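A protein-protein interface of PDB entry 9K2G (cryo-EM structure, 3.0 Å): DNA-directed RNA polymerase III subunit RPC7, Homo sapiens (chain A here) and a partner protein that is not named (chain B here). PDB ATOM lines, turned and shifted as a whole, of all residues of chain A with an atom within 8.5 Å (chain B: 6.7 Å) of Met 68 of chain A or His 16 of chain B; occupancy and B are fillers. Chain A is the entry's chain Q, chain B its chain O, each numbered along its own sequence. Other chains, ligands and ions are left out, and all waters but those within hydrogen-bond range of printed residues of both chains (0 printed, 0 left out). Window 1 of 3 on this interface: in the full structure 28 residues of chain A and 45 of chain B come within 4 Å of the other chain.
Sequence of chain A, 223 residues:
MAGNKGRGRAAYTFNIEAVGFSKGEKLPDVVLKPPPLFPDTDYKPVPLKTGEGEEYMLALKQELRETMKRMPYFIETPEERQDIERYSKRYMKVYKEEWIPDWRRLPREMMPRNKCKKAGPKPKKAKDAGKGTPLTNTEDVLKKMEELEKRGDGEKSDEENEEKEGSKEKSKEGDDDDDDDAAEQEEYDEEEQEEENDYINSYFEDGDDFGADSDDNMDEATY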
ATOM      1  N   LYS A  61      -1.753   5.025   2.458  1.00  0.00           N
ATOM      2  CA  LYS A  61      -2.700   5.761   3.292  1.00  0.00           C
ATOM      3  C   LYS A  61      -2.481   7.265   3.184  1.00  0.00           C
ATOM      4  O   LYS A  61      -3.447   8.038   3.083  1.00  0.00           O
ATOM      5  CB  LYS A  61      -2.577   5.307   4.746  1.00  0.00           C
ATOM      6  CG  LYS A  61      -3.572   5.959   5.687  1.00  0.00           C
ATOM      7  CD  LYS A  61      -3.394   5.448   7.105  1.00  0.00           C
ATOM      8  CE  LYS A  61      -4.517   5.931   8.005  1.00  0.00           C
ATOM      9  NZ  LYS A  61      -5.850   5.497   7.500  1.00  0.00           N
ATOM     10  N   GLN A  62      -1.220   7.703   3.198  1.00  0.00           N
ATOM     11  CA  GLN A  62      -0.941   9.127   3.029  1.00  0.00           C
ATOM     12  C   GLN A  62      -1.387   9.620   1.656  1.00  0.00           C
ATOM     13  O   GLN A  62      -1.925  10.725   1.525  1.00  0.00           O
ATOM     14  CB  GLN A  62       0.547   9.404   3.249  1.00  0.00           C
ATOM     15  CG  GLN A  62       1.011   9.125   4.672  1.00  0.00           C
ATOM     16  CD  GLN A  62       2.426   9.604   4.927  1.00  0.00           C
ATOM     17  OE1 GLN A  62       3.080  10.150   4.039  1.00  0.00           O
ATOM     18  NE2 GLN A  62       2.907   9.404   6.147  1.00  0.00           N
ATOM     19  N   GLU A  63      -1.172   8.806   0.617  1.00  0.00           N
ATOM     20  CA  GLU A  63      -1.627   9.173  -0.719  1.00  0.00           C
ATOM     21  C   GLU A  63      -3.146   9.293  -0.772  1.00  0.00           C
ATOM     22  O   GLU A  63      -3.681  10.202  -1.416  1.00  0.00           O
ATOM     23  CB  GLU A  63      -1.138   8.151  -1.745  1.00  0.00           C
ATOM     24  CG  GLU A  63       0.357   8.191  -1.999  1.00  0.00           C
ATOM     25  CD  GLU A  63       0.811   7.112  -2.960  1.00  0.00           C
ATOM     26  OE1 GLU A  63      -0.053   6.357  -3.453  1.00  0.00           O
ATOM     27  OE2 GLU A  63       2.028   7.022  -3.229  1.00  0.00           O
ATOM     28  N   LEU A  64      -3.857   8.372  -0.116  1.00  0.00           N
ATOM     29  CA  LEU A  64      -5.312   8.450  -0.067  1.00  0.00           C
ATOM     30  C   LEU A  64      -5.767   9.720   0.644  1.00  0.00           C
ATOM     31  O   LEU A  64      -6.710  10.385   0.199  1.00  0.00           O
ATOM     32  CB  LEU A  64      -5.894   7.215   0.622  1.00  0.00           C
ATOM     33  CG  LEU A  64      -5.717   5.874  -0.085  1.00  0.00           C
ATOM     34  CD1 LEU A  64      -6.586   4.803   0.563  1.00  0.00           C
ATOM     35  CD2 LEU A  64      -6.020   5.993  -1.573  1.00  0.00           C
ATOM     36  N   ARG A  65      -5.105  10.065   1.749  1.00  0.00           N
ATOM     37  CA  ARG A  65      -5.411  11.322   2.431  1.00  0.00           C
ATOM     38  C   ARG A  65      -5.234  12.509   1.494  1.00  0.00           C
ATOM     39  O   ARG A  65      -6.089  13.395   1.424  1.00  0.00           O
ATOM     40  CB  ARG A  65      -4.523  11.489   3.663  1.00  0.00           C
ATOM     41  CG  ARG A  65      -4.946  10.700   4.883  1.00  0.00           C
ATOM     42  CD  ARG A  65      -4.355  11.335   6.132  1.00  0.00           C
ATOM     43  NE  ARG A  65      -4.513  10.504   7.318  1.00  0.00           N
ATOM     44  CZ  ARG A  65      -3.580   9.693   7.789  1.00  0.00           C
ATOM     45  NH1 ARG A  65      -2.405   9.567   7.195  1.00  0.00           N
ATOM     46  NH2 ARG A  65      -3.830   8.986   8.889  1.00  0.00           N
ATOM     47  N   GLU A  66      -4.118  12.534   0.761  1.00  0.00           N
ATOM     48  CA  GLU A  66      -3.824  13.686  -0.085  1.00  0.00           C
ATOM     49  C   GLU A  66      -4.744  13.761  -1.297  1.00  0.00           C
ATOM     50  O   GLU A  66      -5.049  14.863  -1.767  1.00  0.00           O
ATOM     51  CB  GLU A  66      -2.360  13.653  -0.533  1.00  0.00           C
ATOM     52  CG  GLU A  66      -1.368  13.851   0.599  1.00  0.00           C
ATOM     53  CD  GLU A  66       0.056  14.001   0.106  1.00  0.00           C
ATOM     54  OE1 GLU A  66       0.289  13.828  -1.112  1.00  0.00           O
ATOM     55  OE2 GLU A  66       0.949  14.301   0.931  1.00  0.00           O
ATOM     56  N   THR A  67      -5.197  12.619  -1.815  1.00  0.00           N
ATOM     57  CA  THR A  67      -5.967  12.627  -3.052  1.00  0.00           C
ATOM     58  C   THR A  67      -7.475  12.684  -2.832  1.00  0.00           C
ATOM     59  O   THR A  67      -8.193  13.169  -3.711  1.00  0.00           O
ATOM     60  CB  THR A  67      -5.628  11.396  -3.905  1.00  0.00           C
ATOM     61  OG1 THR A  67      -6.174  11.566  -5.218  1.00  0.00           O
ATOM     62  CG2 THR A  67      -6.204  10.127  -3.291  1.00  0.00           C
ATOM     63  N   MET A  68      -7.979  12.208  -1.692  1.00  0.00           N
ATOM     64  CA  MET A  68      -9.420  12.188  -1.480  1.00  0.00           C
ATOM     65  C   MET A  68      -9.959  13.491  -0.907  1.00  0.00           C
ATOM     66  O   MET A  68     -11.181  13.662  -0.850  1.00  0.00           O
ATOM     67  CB  MET A  68      -9.811  11.017  -0.571  1.00  0.00           C
ATOM     68  CG  MET A  68     -11.199  10.466  -0.863  1.00  0.00           C
ATOM     69  SD  MET A  68     -11.457   8.793  -0.240  1.00  0.00           S
ATOM     70  CE  MET A  68     -11.302   9.051   1.520  1.00  0.00           C
ATOM     71  N   LYS A  69      -9.089  14.408  -0.484  1.00  0.00           N
ATOM     72  CA  LYS A  69      -9.553  15.748  -0.137  1.00  0.00           C
ATOM     73  C   LYS A  69      -9.840  16.576  -1.382  1.00  0.00           C
ATOM     74  O   LYS A  69     -10.777  17.383  -1.381  1.00  0.00           O
ATOM     75  CB  LYS A  69      -8.520  16.464   0.738  1.00  0.00           C
ATOM     76  CG  LYS A  69      -8.243  15.780   2.065  1.00  0.00           C
ATOM     77  CD  LYS A  69      -7.668  16.757   3.081  1.00  0.00           C
ATOM     78  CE  LYS A  69      -6.483  17.516   2.502  1.00  0.00           C
ATOM     79  NZ  LYS A  69      -5.974  18.546   3.449  1.00  0.00           N
ATOM     80  N   ARG A  70      -9.055  16.392  -2.444  1.00  0.00           N
ATOM     81  CA  ARG A  70      -9.319  17.039  -3.722  1.00  0.00           C
ATOM     82  C   ARG A  70     -10.395  16.327  -4.530  1.00  0.00           C
ATOM     83  O   ARG A  70     -10.866  16.886  -5.528  1.00  0.00           O
ATOM     84  CB  ARG A  70      -8.031  17.122  -4.548  1.00  0.00           C
ATOM     85  CG  ARG A  70      -7.023  18.134  -4.047  1.00  0.00           C
ATOM     86  CD  ARG A  70      -5.772  18.146  -4.911  1.00  0.00           C
ATOM     87  NE  ARG A  70      -4.791  17.152  -4.485  1.00  0.00           N
ATOM     88  CZ  ARG A  70      -4.725  15.909  -4.949  1.00  0.00           C
ATOM     89  NH1 ARG A  70      -5.575  15.463  -5.861  1.00  0.00           N
ATOM     90  NH2 ARG A  70      -3.775  15.098  -4.491  1.00  0.00           N
ATOM     91  N   MET A  71     -10.789  15.120  -4.133  1.00  0.00           N
ATOM     92  CA  MET A  71     -11.857  14.423  -4.827  1.00  0.00           C
ATOM     93  C   MET A  71     -13.170  15.189  -4.671  1.00  0.00           C
ATOM     94  O   MET A  71     -13.459  15.709  -3.587  1.00  0.00           O
ATOM     95  CB  MET A  71     -12.008  12.999  -4.282  1.00  0.00           C
ATOM     96  CG  MET A  71     -12.973  12.126  -5.069  1.00  0.00           C
ATOM     97  SD  MET A  71     -12.353  11.698  -6.704  1.00  0.00           S
ATOM     98  CE  MET A  71     -13.863  11.181  -7.513  1.00  0.00           C
ATOM     99  N   PRO A  72     -13.976  15.288  -5.727  1.00  0.00           N
ATOM    100  CA  PRO A  72     -15.247  16.025  -5.615  1.00  0.00           C
ATOM    101  C   PRO A  72     -16.202  15.455  -4.582  1.00  0.00           C
ATOM    102  O   PRO A  72     -17.100  16.177  -4.136  1.00  0.00           O
ATOM    103  CB  PRO A  72     -15.831  15.931  -7.034  1.00  0.00           C
ATOM    104  CG  PRO A  72     -14.636  15.772  -7.912  1.00  0.00           C
ATOM    105  CD  PRO A  72     -13.663  14.938  -7.125  1.00  0.00           C
ATOM    106  N   TYR A  73     -16.048  14.188  -4.191  1.00  0.00           N
ATOM    107  CA  TYR A  73     -16.882  13.640  -3.126  1.00  0.00           C
ATOM    108  C   TYR A  73     -16.658  14.371  -1.811  1.00  0.00           C
ATOM    109  O   TYR A  73     -17.579  14.477  -0.996  1.00  0.00           O
ATOM    110  CB  TYR A  73     -16.615  12.145  -2.959  1.00  0.00           C
ATOM    111  CG  TYR A  73     -17.093  11.301  -4.117  1.00  0.00           C
ATOM    112  CD1 TYR A  73     -18.429  11.304  -4.500  1.00  0.00           C
ATOM    113  CD2 TYR A  73     -16.214  10.488  -4.819  1.00  0.00           C
ATOM    114  CE1 TYR A  73     -18.872  10.534  -5.557  1.00  0.00           C
ATOM    115  CE2 TYR A  73     -16.649   9.712  -5.877  1.00  0.00           C
ATOM    116  CZ  TYR A  73     -17.978   9.739  -6.242  1.00  0.00           C
ATOM    117  OH  TYR A  73     -18.414   8.968  -7.298  1.00  0.00           O
ATOM    118  N   PHE A  74     -15.448  14.877  -1.585  1.00  0.00           N
ATOM    119  CA  PHE A  74     -15.164  15.668  -0.396  1.00  0.00           C
ATOM    120  C   PHE A  74     -15.824  17.031  -0.530  1.00  0.00           C
ATOM    121  O   PHE A  74     -15.262  17.943  -1.143  1.00  0.00           O
ATOM    122  CB  PHE A  74     -13.649  15.817  -0.194  1.00  0.00           C
ATOM    123  CG  PHE A  74     -13.273  16.570   1.056  1.00  0.00           C
ATOM    124  CD1 PHE A  74     -13.105  15.904   2.257  1.00  0.00           C
ATOM    125  CD2 PHE A  74     -13.076  17.944   1.024  1.00  0.00           C
ATOM    126  CE1 PHE A  74     -12.754  16.592   3.404  1.00  0.00           C
ATOM    127  CE2 PHE A  74     -12.725  18.638   2.168  1.00  0.00           C
ATOM    128  CZ  PHE A  74     -12.563  17.957   3.361  1.00  0.00           C
ATOM    129  N   ILE A  75     -17.024  17.179   0.025  1.00  0.00           N
ATOM    130  CA  ILE A  75     -17.751  18.437  -0.075  1.00  0.00           C
ATOM    131  C   ILE A  75     -17.186  19.407   0.961  1.00  0.00           C
ATOM    132  O   ILE A  75     -17.128  19.099   2.154  1.00  0.00           O
ATOM    133  CB  ILE A  75     -19.262  18.224   0.096  1.00  0.00           C
ATOM    134  CG1 ILE A  75     -20.020  19.535  -0.136  1.00  0.00           C
ATOM    135  CG2 ILE A  75     -19.606  17.601   1.451  1.00  0.00           C
ATOM    136  CD1 ILE A  75     -20.004  19.998  -1.578  1.00  0.00           C
ATOM    137  N   LEU B  11     -14.662  10.568  13.353  1.00  0.00           N
ATOM    138  CA  LEU B  11     -13.316  10.943  12.944  1.00  0.00           C
ATOM    139  C   LEU B  11     -13.032  10.516  11.510  1.00  0.00           C
ATOM    140  O   LEU B  11     -12.481  11.295  10.719  1.00  0.00           O
ATOM    141  CB  LEU B  11     -12.285  10.343  13.900  1.00  0.00           C
ATOM    142  CG  LEU B  11     -12.251  10.943  15.308  1.00  0.00           C
ATOM    143  CD1 LEU B  11     -11.162  10.292  16.146  1.00  0.00           C
ATOM    144  CD2 LEU B  11     -12.059  12.448  15.243  1.00  0.00           C
ATOM    145  N   LEU B  12     -13.410   9.287  11.149  1.00  0.00           N
ATOM    146  CA  LEU B  12     -13.160   8.799   9.795  1.00  0.00           C
ATOM    147  C   LEU B  12     -13.917   9.619   8.759  1.00  0.00           C
ATOM    148  O   LEU B  12     -13.360   9.988   7.721  1.00  0.00           O
ATOM    149  CB  LEU B  12     -13.532   7.320   9.687  1.00  0.00           C
ATOM    150  CG  LEU B  12     -12.568   6.326  10.337  1.00  0.00           C
ATOM    151  CD1 LEU B  12     -13.033   4.892  10.089  1.00  0.00           C
ATOM    152  CD2 LEU B  12     -11.156   6.536   9.817  1.00  0.00           C
ATOM    153  N   LEU B  13     -15.195   9.916   9.018  1.00  0.00           N
ATOM    154  CA  LEU B  13     -15.981  10.684   8.059  1.00  0.00           C
ATOM    155  C   LEU B  13     -15.467  12.112   7.930  1.00  0.00           C
ATOM    156  O   LEU B  13     -15.434  12.666   6.826  1.00  0.00           O
ATOM    157  CB  LEU B  13     -17.456  10.674   8.453  1.00  0.00           C
ATOM    158  CG  LEU B  13     -18.196   9.345   8.301  1.00  0.00           C
ATOM    159  CD1 LEU B  13     -19.694   9.540   8.491  1.00  0.00           C
ATOM    160  CD2 LEU B  13     -17.897   8.705   6.953  1.00  0.00           C
ATOM    161  N   GLN B  14     -15.065  12.727   9.051  1.00  0.00           N
ATOM    162  CA  GLN B  14     -14.511  14.075   8.976  1.00  0.00           C
ATOM    163  C   GLN B  14     -13.200  14.089   8.204  1.00  0.00           C
ATOM    164  O   GLN B  14     -12.940  15.011   7.423  1.00  0.00           O
ATOM    165  CB  GLN B  14     -14.312  14.641  10.383  1.00  0.00           C
ATOM    166  CG  GLN B  14     -13.770  16.061  10.398  1.00  0.00           C
ATOM    167  CD  GLN B  14     -13.620  16.616  11.801  1.00  0.00           C
ATOM    168  OE1 GLN B  14     -13.835  15.913  12.787  1.00  0.00           O
ATOM    169  NE2 GLN B  14     -13.247  17.886  11.896  1.00  0.00           N
ATOM    170  N   GLU B  15     -12.358  13.071   8.406  1.00  0.00           N
ATOM    171  CA  GLU B  15     -11.088  13.014   7.696  1.00  0.00           C
ATOM    172  C   GLU B  15     -11.275  12.698   6.218  1.00  0.00           C
ATOM    173  O   GLU B  15     -10.447  13.096   5.390  1.00  0.00           O
ATOM    174  CB  GLU B  15     -10.171  11.981   8.349  1.00  0.00           C
ATOM    175  CG  GLU B  15      -8.727  12.055   7.889  1.00  0.00           C
ATOM    176  CD  GLU B  15      -8.027  13.304   8.386  1.00  0.00           C
ATOM    177  OE1 GLU B  15      -8.281  13.709   9.539  1.00  0.00           O
ATOM    178  OE2 GLU B  15      -7.232  13.889   7.619  1.00  0.00           O
ATOM    179  N   HIS B  16     -12.346  11.985   5.866  1.00  0.00           N
ATOM    180  CA  HIS B  16     -12.495  11.443   4.517  1.00  0.00           C
ATOM    181  C   HIS B  16     -13.505  12.183   3.652  1.00  0.00           C
ATOM    182  O   HIS B  16     -13.379  12.144   2.422  1.00  0.00           O
ATOM    183  CB  HIS B  16     -12.893   9.959   4.591  1.00  0.00           C
ATOM    184  CG  HIS B  16     -11.784   9.063   5.054  1.00  0.00           C
ATOM    185  ND1 HIS B  16     -11.950   7.707   5.241  1.00  0.00           N
ATOM    186  CD2 HIS B  16     -10.495   9.326   5.360  1.00  0.00           C
ATOM    187  CE1 HIS B  16     -10.811   7.177   5.640  1.00  0.00           C
ATOM    188  NE2 HIS B  16      -9.908   8.136   5.725  1.00  0.00           N
ATOM    189  N   PHE B  17     -14.500  12.847   4.237  1.00  0.00           N
ATOM    190  CA  PHE B  17     -15.577  13.403   3.422  1.00  0.00           C
ATOM    191  C   PHE B  17     -15.859  14.872   3.710  1.00  0.00           C
ATOM    192  O   PHE B  17     -16.277  15.610   2.811  1.00  0.00           O
ATOM    193  CB  PHE B  17     -16.840  12.567   3.608  1.00  0.00           C
ATOM    194  CG  PHE B  17     -16.780  11.219   2.959  1.00  0.00           C
ATOM    195  CD1 PHE B  17     -16.309  11.079   1.660  1.00  0.00           C
ATOM    196  CD2 PHE B  17     -17.186  10.083   3.641  1.00  0.00           C
ATOM    197  CE1 PHE B  17     -16.251   9.839   1.058  1.00  0.00           C
ATOM    198  CE2 PHE B  17     -17.124   8.838   3.042  1.00  0.00           C
ATOM    199  CZ  PHE B  17     -16.659   8.717   1.753  1.00  0.00           C
ATOM    200  N   GLY B  18     -15.636  15.313   4.943  1.00  0.00           N
ATOM    201  CA  GLY B  18     -15.849  16.702   5.279  1.00  0.00           C
ATOM    202  C   GLY B  18     -16.599  16.837   6.585  1.00  0.00           C
ATOM    203  O   GLY B  18     -16.652  15.900   7.390  1.00  0.00           O
ATOM    204  N   VAL B  21     -21.081  16.588   5.970  1.00  0.00           N
ATOM    205  CA  VAL B  21     -21.445  15.214   5.666  1.00  0.00           C
ATOM    206  C   VAL B  21     -21.200  14.295   6.855  1.00  0.00           C
ATOM    207  O   VAL B  21     -21.984  13.375   7.107  1.00  0.00           O
ATOM    208  CB  VAL B  21     -20.683  14.733   4.413  1.00  0.00           C
ATOM    209  CG1 VAL B  21     -19.201  15.058   4.531  1.00  0.00           C
ATOM    210  CG2 VAL B  21     -20.905  13.248   4.181  1.00  0.00           C
ATOM    211  N   HIS B  60     -21.008   5.957  -1.701  1.00  0.00           N
ATOM    212  CA  HIS B  60     -19.989   5.085  -1.132  1.00  0.00           C
ATOM    213  C   HIS B  60     -20.581   3.912  -0.355  1.00  0.00           C
ATOM    214  O   HIS B  60     -19.859   3.265   0.411  1.00  0.00           O
ATOM    215  CB  HIS B  60     -19.051   5.890  -0.229  1.00  0.00           C
ATOM    216  CG  HIS B  60     -18.108   6.779  -0.983  1.00  0.00           C
ATOM    217  ND1 HIS B  60     -18.396   8.099  -1.261  1.00  0.00           N
ATOM    218  CD2 HIS B  60     -16.889   6.539  -1.515  1.00  0.00           C
ATOM    219  CE1 HIS B  60     -17.388   8.633  -1.932  1.00  0.00           C
ATOM    220  NE2 HIS B  60     -16.464   7.706  -2.101  1.00  0.00           N
ATOM    221  N   VAL B  82     -18.793   1.799   7.628  1.00  0.00           N
ATOM    222  CA  VAL B  82     -17.962   2.967   7.906  1.00  0.00           C
ATOM    223  C   VAL B  82     -16.695   2.552   8.641  1.00  0.00           C
ATOM    224  O   VAL B  82     -15.617   3.114   8.413  1.00  0.00           O
ATOM    225  CB  VAL B  82     -18.767   4.016   8.694  1.00  0.00           C
ATOM    226  CG1 VAL B  82     -17.962   5.291   8.822  1.00  0.00           C
ATOM    227  CG2 VAL B  82     -20.102   4.284   8.011  1.00  0.00           C
ATOM    228  N   MET B  85     -14.196   1.097   6.312  1.00  0.00           N
ATOM    229  CA  MET B  85     -13.442   2.088   5.543  1.00  0.00           C
ATOM    230  C   MET B  85     -11.979   2.154   5.986  1.00  0.00           C
ATOM    231  O   MET B  85     -11.100   2.462   5.170  1.00  0.00           O
ATOM    232  CB  MET B  85     -14.094   3.467   5.674  1.00  0.00           C
ATOM    233  CG  MET B  85     -13.343   4.582   4.969  1.00  0.00           C
ATOM    234  SD  MET B  85     -14.189   6.173   5.065  1.00  0.00           S
ATOM    235  CE  MET B  85     -15.732   5.792   4.240  1.00  0.00           C
ATOM    236  N   LEU B  86     -11.685   1.838   7.253  1.00  0.00           N
ATOM    237  CA  LEU B  86     -10.311   1.907   7.747  1.00  0.00           C
ATOM    238  C   LEU B  86      -9.406   0.839   7.138  1.00  0.00           C
ATOM    239  O   LEU B  86      -8.184   1.016   7.132  1.00  0.00           O
ATOM    240  CB  LEU B  86     -10.290   1.788   9.271  1.00  0.00           C
ATOM    241  CG  LEU B  86      -8.960   2.021   9.992  1.00  0.00           C
ATOM    242  CD1 LEU B  86      -8.448   3.416   9.685  1.00  0.00           C
ATOM    243  CD2 LEU B  86      -9.117   1.822  11.491  1.00  0.00           C
ATOM    244  N   TYR B  88      -9.076   0.056   4.055  1.00  0.00           N
ATOM    245  CA  TYR B  88      -8.758   0.327   2.654  1.00  0.00           C
ATOM    246  C   TYR B  88      -7.290   0.113   2.303  1.00  0.00           C
ATOM    247  O   TYR B  88      -7.017  -0.535   1.278  1.00  0.00           O
ATOM    248  CB  TYR B  88      -9.206   1.749   2.286  1.00  0.00           C
ATOM    249  CG  TYR B  88     -10.705   1.915   2.146  1.00  0.00           C
ATOM    250  CD1 TYR B  88     -11.555   0.822   2.268  1.00  0.00           C
ATOM    251  CD2 TYR B  88     -11.261   3.154   1.877  1.00  0.00           C
ATOM    252  CE1 TYR B  88     -12.924   0.967   2.137  1.00  0.00           C
ATOM    253  CE2 TYR B  88     -12.629   3.311   1.741  1.00  0.00           C
ATOM    254  CZ  TYR B  88     -13.451   2.215   1.873  1.00  0.00           C
ATOM    255  OH  TYR B  88     -14.815   2.371   1.739  1.00  0.00           O
ATOM    256  N   LEU B 111     -12.791   1.677  -4.382  1.00  0.00           N
ATOM    257  CA  LEU B 111     -12.949   2.114  -2.999  1.00  0.00           C
ATOM    258  C   LEU B 111     -13.078   3.630  -2.897  1.00  0.00           C
ATOM    259  O   LEU B 111     -13.840   4.138  -2.068  1.00  0.00           O
ATOM    260  CB  LEU B 111     -11.774   1.613  -2.155  1.00  0.00           C
ATOM    261  CG  LEU B 111     -11.773   0.111  -1.865  1.00  0.00           C
ATOM    262  CD1 LEU B 111     -10.606  -0.263  -0.971  1.00  0.00           C
ATOM    263  CD2 LEU B 111     -13.091  -0.316  -1.244  1.00  0.00           C
ATOM    264  N   LEU B 112     -12.339   4.371  -3.730  1.00  0.00           N
ATOM    265  CA  LEU B 112     -12.416   5.829  -3.678  1.00  0.00           C
ATOM    266  C   LEU B 112     -13.705   6.370  -4.275  1.00  0.00           C
ATOM    267  O   LEU B 112     -14.096   7.496  -3.952  1.00  0.00           O
ATOM    268  CB  LEU B 112     -11.216   6.448  -4.394  1.00  0.00           C
ATOM    269  CG  LEU B 112     -10.027   6.858  -3.519  1.00  0.00           C
ATOM    270  CD1 LEU B 112      -9.406   5.643  -2.843  1.00  0.00           C
ATOM    271  CD2 LEU B 112      -8.997   7.620  -4.337  1.00  0.00           C
ATOM    272  N   ASN B 113     -14.380   5.602  -5.134  1.00  0.00           N
ATOM    273  CA  ASN B 113     -15.613   6.060  -5.755  1.00  0.00           C
ATOM    274  C   ASN B 113     -16.848   5.287  -5.314  1.00  0.00           C
ATOM    275  O   ASN B 113     -17.970   5.741  -5.575  1.00  0.00           O
ATOM    276  CB  ASN B 113     -15.492   5.990  -7.285  1.00  0.00           C
ATOM    277  CG  ASN B 113     -14.409   6.901  -7.827  1.00  0.00           C
ATOM    278  OD1 ASN B 113     -14.689   7.993  -8.314  1.00  0.00           O
ATOM    279  ND2 ASN B 113     -13.161   6.450  -7.745  1.00  0.00           N
ATOM    280  N   GLU B 513      -2.030   2.808  13.802  1.00  0.00           N
ATOM    281  CA  GLU B 513      -3.455   2.798  13.500  1.00  0.00           C
ATOM    282  C   GLU B 513      -3.799   1.695  12.511  1.00  0.00           C
ATOM    283  O   GLU B 513      -4.842   1.041  12.629  1.00  0.00           O
ATOM    284  CB  GLU B 513      -3.873   4.167  12.961  1.00  0.00           C
ATOM    285  CG  GLU B 513      -5.241   4.227  12.323  1.00  0.00           C
ATOM    286  CD  GLU B 513      -5.510   5.571  11.669  1.00  0.00           C
ATOM    287  OE1 GLU B 513      -4.889   6.570  12.091  1.00  0.00           O
ATOM    288  OE2 GLU B 513      -6.336   5.629  10.733  1.00  0.00           O
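O of Leu 13 of chain B is in hydrogen-bond range of N of Gly 18 of chain B (3.3 Å).
A ring nitrogen (ND1) of His 16 of chain B sits at hydrogen-bond distance from the side-chain sulfur of Met 85 of chain B (2.7 Å).
A ring nitrogen (NE2) of His 60 of chain B is in hydrogen-bond range of the backbone carbonyl oxygen of Leu 112 of chain B, 3.0 Å away.
Met 68 of chain A touches just one residue of chain B: His 16 (3.6 Å).
His 16 of chain B touches two residues of chain A.
Printed residues of chain A within 4 Å of Gly 18 of chain B: Phe 74 (3.5 Å).
Printed residues of chain A within 4 Å of Asn 113 of chain B: Met 71 (3.4 Å) and Tyr 73 (3.6 Å).
Of the printed residues of chain A, Leu 112 of chain B touches Leu 64 (3.6 Å), Thr 67 (3.9 Å) and Tyr 73 (3.8 Å).
Of the printed residues of chain A, His 60 of chain B touches Tyr 73.
Tyr 88 of chain B touches none of the printed residues of chain A.
Glu 63 of chain A touches none of the printed residues of chain B.
The nearest residue of chain B that does not touch Met 68 of chain A is Leu 112 of chain B (4.1 Å).
The nearest residue of chain A that does not touch His 16 of chain B is Lys 61 of chain A (5.2 Å).
The nearest printed residue of chain B that does not touch Met 71 of chain A is Leu 112 of chain B (4.9 Å).
Leu 86 of chain B touches Lys 61 of chain A (CD1 to NZ, 3.98 Å).
Leu 112 of chain B touches Leu 64 of chain A (CD1 to CD2, 3.6 Å).
Thr 67 of chain A touches Leu 112 of chain B (CG2 to CD2, 3.9 Å).
CE of Met 68 of chain A touches CG of His 16 of chain B, 3.6 Å away.
Asn 113 of chain B touches Met 71 of chain A (OD1 to CE, 3.4 Å).
CG of Tyr 73 of chain A touches CE1 of His 60 of chain B, at 3.5 Å.
Tyr 73 of chain A touches Leu 112 of chain B.
OD1 of Asn 113 of chain B touches CE2 of Tyr 73 of chain A, at 3.6 Å.
O of Phe 17 of chain B touches CD1 of Phe 74 of chain A (3.2 Å).
Phe 74 of chain A touches Gly 18 of chain B (CE1 to N, 3.5 Å).
Of the 18 printed residues of chain B, 8 touch a printed residue of chain A.
Hydrophobic or aromatic side chains of chain B that line the printed part of chain A: His 16, His 60, Leu 86 and Leu 112.
Of the 15 printed residues of chain A, 8 touch a printed residue of chain B.
Hydrophobic or aromatic side chains of chain A that line the printed part of chain B: Leu 64, Met 68, Met 71, Tyr 73 and Phe 74.
Among the printed residues, Asp or Glu carboxylates within 4 Å of a Lys or Arg side-chain nitrogen of the other chain: Lys 61 of chain A with Glu 513 of chain B.
O of Phe 17 of chain B sits at hydrogen-bond distance from N of Ile 75 of chain A (3.3 Å).
The side-chain carboxylate (OE2) of Glu 513 of chain B is in salt-bridge range of the side-chain amino group (NZ) of Lys 61 of chain A, at 3.3 Å.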
